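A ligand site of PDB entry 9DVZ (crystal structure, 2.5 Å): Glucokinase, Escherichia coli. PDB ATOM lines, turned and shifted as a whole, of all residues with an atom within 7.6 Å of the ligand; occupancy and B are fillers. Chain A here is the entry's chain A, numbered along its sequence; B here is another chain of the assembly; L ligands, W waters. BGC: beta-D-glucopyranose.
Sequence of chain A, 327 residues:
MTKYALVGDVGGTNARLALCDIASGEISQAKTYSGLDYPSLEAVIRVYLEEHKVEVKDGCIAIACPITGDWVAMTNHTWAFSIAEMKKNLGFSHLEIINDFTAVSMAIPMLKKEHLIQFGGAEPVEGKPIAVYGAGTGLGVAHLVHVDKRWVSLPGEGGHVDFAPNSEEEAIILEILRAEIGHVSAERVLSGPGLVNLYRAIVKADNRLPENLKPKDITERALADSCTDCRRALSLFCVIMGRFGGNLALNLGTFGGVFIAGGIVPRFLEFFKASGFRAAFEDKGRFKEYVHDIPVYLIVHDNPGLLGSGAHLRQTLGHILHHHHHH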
ATOM      1  N   VAL A  10      15.298 -36.422  24.719  1.00  0.00           N
ATOM      2  CA  VAL A  10      15.768 -35.596  25.825  1.00  0.00           C
ATOM      3  C   VAL A  10      14.821 -34.415  25.967  1.00  0.00           C
ATOM      4  O   VAL A  10      14.552 -33.694  24.994  1.00  0.00           O
ATOM      5  CB  VAL A  10      17.211 -35.122  25.597  1.00  0.00           C
ATOM      6  CG1 VAL A  10      17.702 -34.313  26.780  1.00  0.00           C
ATOM      7  CG2 VAL A  10      18.122 -36.306  25.336  1.00  0.00           C
ATOM      8  N   GLY A  11      14.324 -34.197  27.177  1.00  0.00           N
ATOM      9  CA  GLY A  11      13.493 -33.035  27.441  1.00  0.00           C
ATOM     10  C   GLY A  11      13.484 -32.611  28.894  1.00  0.00           C
ATOM     11  O   GLY A  11      13.235 -33.432  29.784  1.00  0.00           O
ATOM     12  N   ILE A  63      15.398 -33.676  20.958  1.00  0.00           N
ATOM     13  CA  ILE A  63      15.519 -32.748  22.079  1.00  0.00           C
ATOM     14  C   ILE A  63      14.419 -31.699  21.977  1.00  0.00           C
ATOM     15  O   ILE A  63      14.131 -31.194  20.893  1.00  0.00           O
ATOM     16  CB  ILE A  63      16.914 -32.082  22.120  1.00  0.00           C
ATOM     17  CG1 ILE A  63      18.016 -33.142  22.155  1.00  0.00           C
ATOM     18  CG2 ILE A  63      17.031 -31.166  23.326  1.00  0.00           C
ATOM     19  CD1 ILE A  63      19.301 -32.713  21.491  1.00  0.00           C
ATOM     20  N   ALA A  64      13.815 -31.373  23.117  1.00  0.00           N
ATOM     21  CA  ALA A  64      12.673 -30.462  23.173  1.00  0.00           C
ATOM     22  C   ALA A  64      13.155 -29.012  23.187  1.00  0.00           C
ATOM     23  O   ALA A  64      13.079 -28.287  24.189  1.00  0.00           O
ATOM     24  CB  ALA A  64      11.821 -30.771  24.396  1.00  0.00           C
ATOM     25  N   CYS A  65      13.655 -28.575  22.031  1.00  0.00           N
ATOM     26  CA  CYS A  65      14.041 -27.189  21.799  1.00  0.00           C
ATOM     27  C   CYS A  65      14.196 -26.996  20.295  1.00  0.00           C
ATOM     28  O   CYS A  65      14.276 -27.973  19.542  1.00  0.00           O
ATOM     29  CB  CYS A  65      15.348 -26.839  22.544  1.00  0.00           C
ATOM     30  SG  CYS A  65      16.819 -27.743  22.001  1.00  0.00           S
ATOM     31  N   PRO A  66      14.212 -25.750  19.817  1.00  0.00           N
ATOM     32  CA  PRO A  66      14.390 -25.526  18.379  1.00  0.00           C
ATOM     33  C   PRO A  66      15.786 -25.962  17.940  1.00  0.00           C
ATOM     34  O   PRO A  66      16.783 -25.631  18.578  1.00  0.00           O
ATOM     35  CB  PRO A  66      14.207 -24.019  18.211  1.00  0.00           C
ATOM     36  CG  PRO A  66      13.556 -23.550  19.464  1.00  0.00           C
ATOM     37  CD  PRO A  66      13.960 -24.497  20.544  1.00  0.00           C
ATOM     38  N   ILE A  67      15.834 -26.708  16.828  1.00  0.00           N
ATOM     39  CA  ILE A  67      17.107 -27.151  16.256  1.00  0.00           C
ATOM     40  C   ILE A  67      17.338 -26.341  14.989  1.00  0.00           C
ATOM     41  O   ILE A  67      16.883 -26.713  13.899  1.00  0.00           O
ATOM     42  CB  ILE A  67      17.097 -28.660  15.953  1.00  0.00           C
ATOM     43  CG1 ILE A  67      16.870 -29.500  17.219  1.00  0.00           C
ATOM     44  CG2 ILE A  67      18.411 -29.079  15.312  1.00  0.00           C
ATOM     45  CD1 ILE A  67      17.436 -28.908  18.503  1.00  0.00           C
ATOM     46  N   MET A  74      19.310 -25.837  25.260  1.00  0.00           N
ATOM     47  CA  MET A  74      17.976 -26.343  25.616  1.00  0.00           C
ATOM     48  C   MET A  74      17.102 -25.267  26.236  1.00  0.00           C
ATOM     49  O   MET A  74      15.902 -25.193  25.944  1.00  0.00           O
ATOM     50  CB  MET A  74      18.109 -27.539  26.549  1.00  0.00           C
ATOM     51  CG  MET A  74      18.666 -28.778  25.870  1.00  0.00           C
ATOM     52  SD  MET A  74      18.488 -30.262  26.876  1.00  0.00           S
ATOM     53  CE  MET A  74      20.183 -30.823  26.934  1.00  0.00           C
ATOM     54  N   ASN A  76      15.700 -25.170  28.799  1.00  0.00           N
ATOM     55  CA  ASN A  76      14.993 -25.853  29.868  1.00  0.00           C
ATOM     56  C   ASN A  76      15.940 -26.709  30.702  1.00  0.00           C
ATOM     57  O   ASN A  76      15.492 -27.482  31.552  1.00  0.00           O
ATOM     58  CB  ASN A  76      13.858 -26.716  29.303  1.00  0.00           C
ATOM     59  CG  ASN A  76      12.501 -26.332  29.866  1.00  0.00           C
ATOM     60  OD1 ASN A  76      12.221 -25.151  30.078  1.00  0.00           O
ATOM     61  ND2 ASN A  76      11.661 -27.319  30.104  1.00  0.00           N
ATOM     62  N   ASN A  99      14.301 -31.949  16.681  1.00  0.00           N
ATOM     63  CA  ASN A  99      13.312 -31.480  17.646  1.00  0.00           C
ATOM     64  C   ASN A  99      12.410 -32.635  18.084  1.00  0.00           C
ATOM     65  O   ASN A  99      12.157 -33.566  17.318  1.00  0.00           O
ATOM     66  CB  ASN A  99      12.491 -30.339  17.035  1.00  0.00           C
ATOM     67  CG  ASN A  99      11.292 -29.960  17.878  1.00  0.00           C
ATOM     68  OD1 ASN A  99      10.175 -30.428  17.632  1.00  0.00           O
ATOM     69  ND2 ASN A  99      11.508 -29.127  18.877  1.00  0.00           N
ATOM     70  N   ASP A 100      11.931 -32.556  19.328  1.00  0.00           N
ATOM     71  CA  ASP A 100      11.243 -33.706  19.907  1.00  0.00           C
ATOM     72  C   ASP A 100       9.945 -34.036  19.180  1.00  0.00           C
ATOM     73  O   ASP A 100       9.529 -35.204  19.191  1.00  0.00           O
ATOM     74  CB  ASP A 100      10.951 -33.470  21.395  1.00  0.00           C
ATOM     75  CG  ASP A 100      10.063 -32.275  21.633  1.00  0.00           C
ATOM     76  OD1 ASP A 100      10.053 -31.361  20.787  1.00  0.00           O
ATOM     77  OD2 ASP A 100       9.365 -32.266  22.664  1.00  0.00           O
ATOM     78  N   PHE A 101       9.300 -33.069  18.552  1.00  0.00           N
ATOM     79  CA  PHE A 101       8.080 -33.375  17.831  1.00  0.00           C
ATOM     80  C   PHE A 101       8.319 -33.669  16.355  1.00  0.00           C
ATOM     81  O   PHE A 101       7.407 -34.172  15.692  1.00  0.00           O
ATOM     82  CB  PHE A 101       7.053 -32.255  18.001  1.00  0.00           C
ATOM     83  CG  PHE A 101       6.103 -32.501  19.123  1.00  0.00           C
ATOM     84  CD1 PHE A 101       6.568 -32.506  20.427  1.00  0.00           C
ATOM     85  CD2 PHE A 101       4.770 -32.808  18.892  1.00  0.00           C
ATOM     86  CE1 PHE A 101       5.718 -32.754  21.486  1.00  0.00           C
ATOM     87  CE2 PHE A 101       3.911 -33.060  19.949  1.00  0.00           C
ATOM     88  CZ  PHE A 101       4.389 -33.036  21.236  1.00  0.00           C
ATOM     89  N   THR A 102       9.506 -33.374  15.835  1.00  0.00           N
ATOM     90  CA  THR A 102       9.945 -34.027  14.606  1.00  0.00           C
ATOM     91  C   THR A 102       9.984 -35.534  14.790  1.00  0.00           C
ATOM     92  O   THR A 102       9.496 -36.288  13.946  1.00  0.00           O
ATOM     93  CB  THR A 102      11.316 -33.498  14.196  1.00  0.00           C
ATOM     94  OG1 THR A 102      11.287 -32.066  14.119  1.00  0.00           O
ATOM     95  CG2 THR A 102      11.734 -34.067  12.843  1.00  0.00           C
ATOM     96  N   GLY A 134       1.124 -31.766  20.941  1.00  0.00           N
ATOM     97  CA  GLY A 134       1.099 -32.374  22.256  1.00  0.00           C
ATOM     98  C   GLY A 134       1.368 -31.395  23.380  1.00  0.00           C
ATOM     99  O   GLY A 134       2.271 -30.558  23.280  1.00  0.00           O
ATOM    100  N   ALA A 135       0.594 -31.508  24.451  1.00  0.00           N
ATOM    101  CA  ALA A 135       0.745 -30.634  25.612  1.00  0.00           C
ATOM    102  C   ALA A 135       1.482 -31.404  26.705  1.00  0.00           C
ATOM    103  O   ALA A 135       0.946 -32.351  27.276  1.00  0.00           O
ATOM    104  CB  ALA A 135      -0.622 -30.149  26.105  1.00  0.00           C
ATOM    105  N   GLY A 136       2.707 -30.983  26.982  1.00  0.00           N
ATOM    106  CA  GLY A 136       3.513 -31.578  28.043  1.00  0.00           C
ATOM    107  C   GLY A 136       4.154 -30.514  28.921  1.00  0.00           C
ATOM    108  O   GLY A 136       3.464 -29.675  29.493  1.00  0.00           O
ATOM    109  N   THR A 137       5.484 -30.566  29.042  1.00  0.00           N
ATOM    110  CA  THR A 137       6.199 -29.459  29.656  1.00  0.00           C
ATOM    111  C   THR A 137       6.080 -28.195  28.796  1.00  0.00           C
ATOM    112  O   THR A 137       5.938 -27.090  29.322  1.00  0.00           O
ATOM    113  CB  THR A 137       7.660 -29.842  29.886  1.00  0.00           C
ATOM    114  OG1 THR A 137       7.734 -30.823  30.919  1.00  0.00           O
ATOM    115  CG2 THR A 137       8.482 -28.622  30.321  1.00  0.00           C
ATOM    116  N   GLY A 138       6.127 -28.362  27.478  1.00  0.00           N
ATOM    117  CA  GLY A 138       5.831 -27.296  26.541  1.00  0.00           C
ATOM    118  C   GLY A 138       4.774 -27.751  25.552  1.00  0.00           C
ATOM    119  O   GLY A 138       4.233 -28.855  25.689  1.00  0.00           O
ATOM    120  N   LEU A 139       4.467 -26.924  24.562  1.00  0.00           N
ATOM    121  CA  LEU A 139       3.515 -27.258  23.512  1.00  0.00           C
ATOM    122  C   LEU A 139       4.288 -27.517  22.221  1.00  0.00           C
ATOM    123  O   LEU A 139       4.852 -26.590  21.627  1.00  0.00           O
ATOM    124  CB  LEU A 139       2.493 -26.136  23.325  1.00  0.00           C
ATOM    125  CG  LEU A 139       1.421 -26.335  22.246  1.00  0.00           C
ATOM    126  CD1 LEU A 139       0.748 -27.687  22.401  1.00  0.00           C
ATOM    127  CD2 LEU A 139       0.392 -25.223  22.312  1.00  0.00           C
ATOM    128  N   GLY A 140       4.311 -28.779  21.795  1.00  0.00           N
ATOM    129  CA  GLY A 140       4.994 -29.173  20.577  1.00  0.00           C
ATOM    130  C   GLY A 140       4.017 -29.313  19.422  1.00  0.00           C
ATOM    131  O   GLY A 140       2.888 -29.743  19.614  1.00  0.00           O
ATOM    132  N   VAL A 141       4.469 -28.902  18.237  1.00  0.00           N
ATOM    133  CA  VAL A 141       3.687 -29.020  17.008  1.00  0.00           C
ATOM    134  C   VAL A 141       4.621 -29.408  15.881  1.00  0.00           C
ATOM    135  O   VAL A 141       5.714 -28.843  15.740  1.00  0.00           O
ATOM    136  CB  VAL A 141       2.943 -27.704  16.668  1.00  0.00           C
ATOM    137  CG1 VAL A 141       2.420 -27.744  15.238  1.00  0.00           C
ATOM    138  CG2 VAL A 141       1.804 -27.461  17.634  1.00  0.00           C
ATOM    139  N   ALA A 142       4.203 -30.378  15.072  1.00  0.00           N
ATOM    140  CA  ALA A 142       4.913 -30.735  13.855  1.00  0.00           C
ATOM    141  C   ALA A 142       3.903 -31.186  12.820  1.00  0.00           C
ATOM    142  O   ALA A 142       2.757 -31.497  13.138  1.00  0.00           O
ATOM    143  CB  ALA A 142       5.971 -31.820  14.096  1.00  0.00           C
ATOM    144  N   GLY A 156       8.613 -27.178  13.424  1.00  0.00           N
ATOM    145  CA  GLY A 156       8.341 -25.774  13.688  1.00  0.00           C
ATOM    146  C   GLY A 156       8.234 -25.540  15.178  1.00  0.00           C
ATOM    147  O   GLY A 156       8.391 -26.453  15.995  1.00  0.00           O
ATOM    148  N   GLU A 157       7.958 -24.284  15.526  1.00  0.00           N
ATOM    149  CA  GLU A 157       7.733 -23.878  16.910  1.00  0.00           C
ATOM    150  C   GLU A 157       6.301 -23.390  17.088  1.00  0.00           C
ATOM    151  O   GLU A 157       6.044 -22.388  17.762  1.00  0.00           O
ATOM    152  CB  GLU A 157       8.729 -22.794  17.308  1.00  0.00           C
ATOM    153  CG  GLU A 157      10.171 -23.279  17.337  1.00  0.00           C
ATOM    154  CD  GLU A 157      10.401 -24.373  18.358  1.00  0.00           C
ATOM    155  OE1 GLU A 157      10.006 -24.194  19.526  1.00  0.00           O
ATOM    156  OE2 GLU A 157      10.968 -25.420  17.991  1.00  0.00           O
ATOM    157  N   GLY A 158       5.346 -24.123  16.510  1.00  0.00           N
ATOM    158  CA  GLY A 158       3.956 -23.701  16.454  1.00  0.00           C
ATOM    159  C   GLY A 158       3.283 -23.602  17.811  1.00  0.00           C
ATOM    160  O   GLY A 158       2.168 -23.065  17.887  1.00  0.00           O
ATOM    161  N   GLY A 159       3.908 -24.097  18.877  1.00  0.00           N
ATOM    162  CA  GLY A 159       3.351 -23.911  20.195  1.00  0.00           C
ATOM    163  C   GLY A 159       3.465 -22.501  20.729  1.00  0.00           C
ATOM    164  O   GLY A 159       2.833 -22.189  21.751  1.00  0.00           O
ATOM    165  N   HIS A 160       4.248 -21.650  20.075  1.00  0.00           N
ATOM    166  CA  HIS A 160       4.488 -20.278  20.522  1.00  0.00           C
ATOM    167  C   HIS A 160       3.724 -19.242  19.693  1.00  0.00           C
ATOM    168  O   HIS A 160       4.034 -18.050  19.767  1.00  0.00           O
ATOM    169  CB  HIS A 160       5.981 -19.977  20.522  1.00  0.00           C
ATOM    170  CG  HIS A 160       6.771 -20.910  21.399  1.00  0.00           C
ATOM    171  ND1 HIS A 160       6.842 -20.752  22.769  1.00  0.00           N
ATOM    172  CD2 HIS A 160       7.513 -21.999  21.110  1.00  0.00           C
ATOM    173  CE1 HIS A 160       7.593 -21.704  23.278  1.00  0.00           C
ATOM    174  NE2 HIS A 160       8.016 -22.476  22.286  1.00  0.00           N
ATOM    175  N   GLU A 187       1.189 -22.053  24.359  1.00  0.00           N
ATOM    176  CA  GLU A 187       1.863 -22.827  25.392  1.00  0.00           C
ATOM    177  C   GLU A 187       1.471 -22.377  26.795  1.00  0.00           C
ATOM    178  O   GLU A 187       1.401 -23.200  27.714  1.00  0.00           O
ATOM    179  CB  GLU A 187       3.369 -22.715  25.202  1.00  0.00           C
ATOM    180  CG  GLU A 187       4.206 -23.513  26.194  1.00  0.00           C
ATOM    181  CD  GLU A 187       5.671 -23.586  25.785  1.00  0.00           C
ATOM    182  OE1 GLU A 187       6.026 -24.498  25.010  1.00  0.00           O
ATOM    183  OE2 GLU A 187       6.459 -22.731  26.235  1.00  0.00           O
ATOM    184  N   ARG B 286       9.395 -14.742  23.775  1.00  0.00           N
ATOM    185  CA  ARG B 286      10.742 -15.296  23.733  1.00  0.00           C
ATOM    186  C   ARG B 286      11.175 -15.710  22.327  1.00  0.00           C
ATOM    187  O   ARG B 286      12.361 -15.982  22.123  1.00  0.00           O
ATOM    188  CB  ARG B 286      10.854 -16.511  24.652  1.00  0.00           C
ATOM    189  CG  ARG B 286      10.427 -16.252  26.079  1.00  0.00           C
ATOM    190  CD  ARG B 286      10.134 -17.549  26.813  1.00  0.00           C
ATOM    191  NE  ARG B 286       8.875 -18.150  26.364  1.00  0.00           N
ATOM    192  CZ  ARG B 286       8.441 -19.343  26.741  1.00  0.00           C
ATOM    193  NH1 ARG B 286       9.117 -20.089  27.594  1.00  0.00           N
ATOM    194  NH2 ARG B 286       7.285 -19.784  26.254  1.00  0.00           N
ATOM    195  N   PHE B 287      10.244 -15.781  21.378  1.00  0.00           N
ATOM    196  CA  PHE B 287      10.557 -16.243  20.034  1.00  0.00           C
ATOM    197  C   PHE B 287      10.540 -15.113  19.017  1.00  0.00           C
ATOM    198  O   PHE B 287      10.341 -15.364  17.822  1.00  0.00           O
ATOM    199  CB  PHE B 287       9.597 -17.356  19.644  1.00  0.00           C
ATOM    200  CG  PHE B 287      10.035 -18.705  20.140  1.00  0.00           C
ATOM    201  CD1 PHE B 287       9.826 -19.056  21.468  1.00  0.00           C
ATOM    202  CD2 PHE B 287      10.669 -19.606  19.303  1.00  0.00           C
ATOM    203  CE1 PHE B 287      10.240 -20.276  21.937  1.00  0.00           C
ATOM    204  CE2 PHE B 287      11.075 -20.831  19.769  1.00  0.00           C
ATOM    205  CZ  PHE B 287      10.864 -21.175  21.090  1.00  0.00           C
HETATM  206  C2  BGC L   1       9.773 -25.929  22.540  1.00  0.00           C
HETATM  207  C3  BGC L   1       9.666 -26.807  21.353  1.00  0.00           C
HETATM  208  C4  BGC L   1       9.208 -28.179  21.735  1.00  0.00           C
HETATM  209  C5  BGC L   1       7.891 -28.133  22.499  1.00  0.00           C
HETATM  210  C6  BGC L   1       7.498 -29.534  22.911  1.00  0.00           C
HETATM  211  C1  BGC L   1       8.460 -25.874  23.313  1.00  0.00           C
HETATM  212  O1  BGC L   1       8.601 -25.118  24.435  1.00  0.00           O
HETATM  213  O2  BGC L   1      10.123 -24.591  22.107  1.00  0.00           O
HETATM  214  O3  BGC L   1      10.965 -26.894  20.691  1.00  0.00           O
HETATM  215  O4  BGC L   1       9.035 -28.947  20.538  1.00  0.00           O
HETATM  216  O5  BGC L   1       7.960 -27.251  23.685  1.00  0.00           O
HETATM  217  O6  BGC L   1       8.450 -30.084  23.778  1.00  0.00           O
HETATM  218  O   HOH W   1      10.496 -22.965  25.154  1.00  0.00           O
HETATM  219  O   HOH W   2       7.586 -27.705  18.444  1.00  0.00           O
HETATM  220  O   HOH W   3      12.274 -23.781  23.131  1.00  0.00           O
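O2 of the ligand sits at hydrogen-bond distance from OE1 of Glu 157, at 2.6 Å. The side-chain amide nitrogen (ND2) of Asn 99 is in hydrogen-bond range of an oxygen (O3) of the ligand (2.9 Å). NE2 of His 160 is in hydrogen-bond range of O2 of the ligand, at 3.0 Å. OE1 of Glu 187 sits at hydrogen-bond distance from O1 of the ligand (2.7 Å). O3 of the ligand lies close to N of Cys 65, at 3.4 Å. The side-chain carboxylate (OD2) of Asp 100 lies within hydrogen-bond range of an oxygen (O6) of the ligand.
The backbone NH (N) of Phe 101 sits at hydrogen-bond distance from the side-chain amide oxygen (OD1) of Asn 99. The side-chain carboxylate (OD1) of Asp 100 sits at hydrogen-bond distance from the side-chain amide nitrogen (ND2) of Asn 99 (3.3 Å). O of Gly 159 lies within hydrogen-bond range of N of Glu 187, at 3.1 Å. The side-chain amide nitrogen (ND2) of Asn 99 is in hydrogen-bond range of the backbone carbonyl oxygen (O) of Cys 65 (3.1 Å). O of Gly 140 is in hydrogen-bond range of N of Gly 134 (3.0 Å). The backbone carbonyl oxygen (O) of Ile 63 sits at hydrogen-bond distance from the backbone NH (N) of Asp 100, 3.0 Å away. N of Leu 139 is in hydrogen-bond range of OE1 of Glu 187, at 2.9 Å. NH2 of Arg 286 of chain B lies within salt-bridge range of OE2 of Glu 187.
Merely in contact with the ligand: Gly 140 (3.4 Å), Ala 64 (3.5 Å), Leu 139 (3.5 Å), Pro 66 (3.6 Å), Gly 138 (3.6 Å), Phe 287 of chain B (3.6 Å) and Phe 101 (3.9 Å). Hydrophobic or aromatic side chains within 4 Å of the ligand: Ala 64, Pro 66, Phe 101, His 160 and Phe 287 of chain B. 13 residues have an atom within 4 Å of the ligand: Ala 64, Cys 65, Pro 66, Asn 99, Asp 100, Phe 101, Gly 138, Leu 139, Gly 140, Glu 157, His 160, Glu 187 and Phe 287 of chain B. The nearest printed residue that does not touch the ligand is Val 141 (5.1 Å).
Water W2 lies within hydrogen-bond range of O4 of the ligand (2.8 Å), O of Gly 156 (2.9 Å) and N of Val 141 (3.3 Å).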
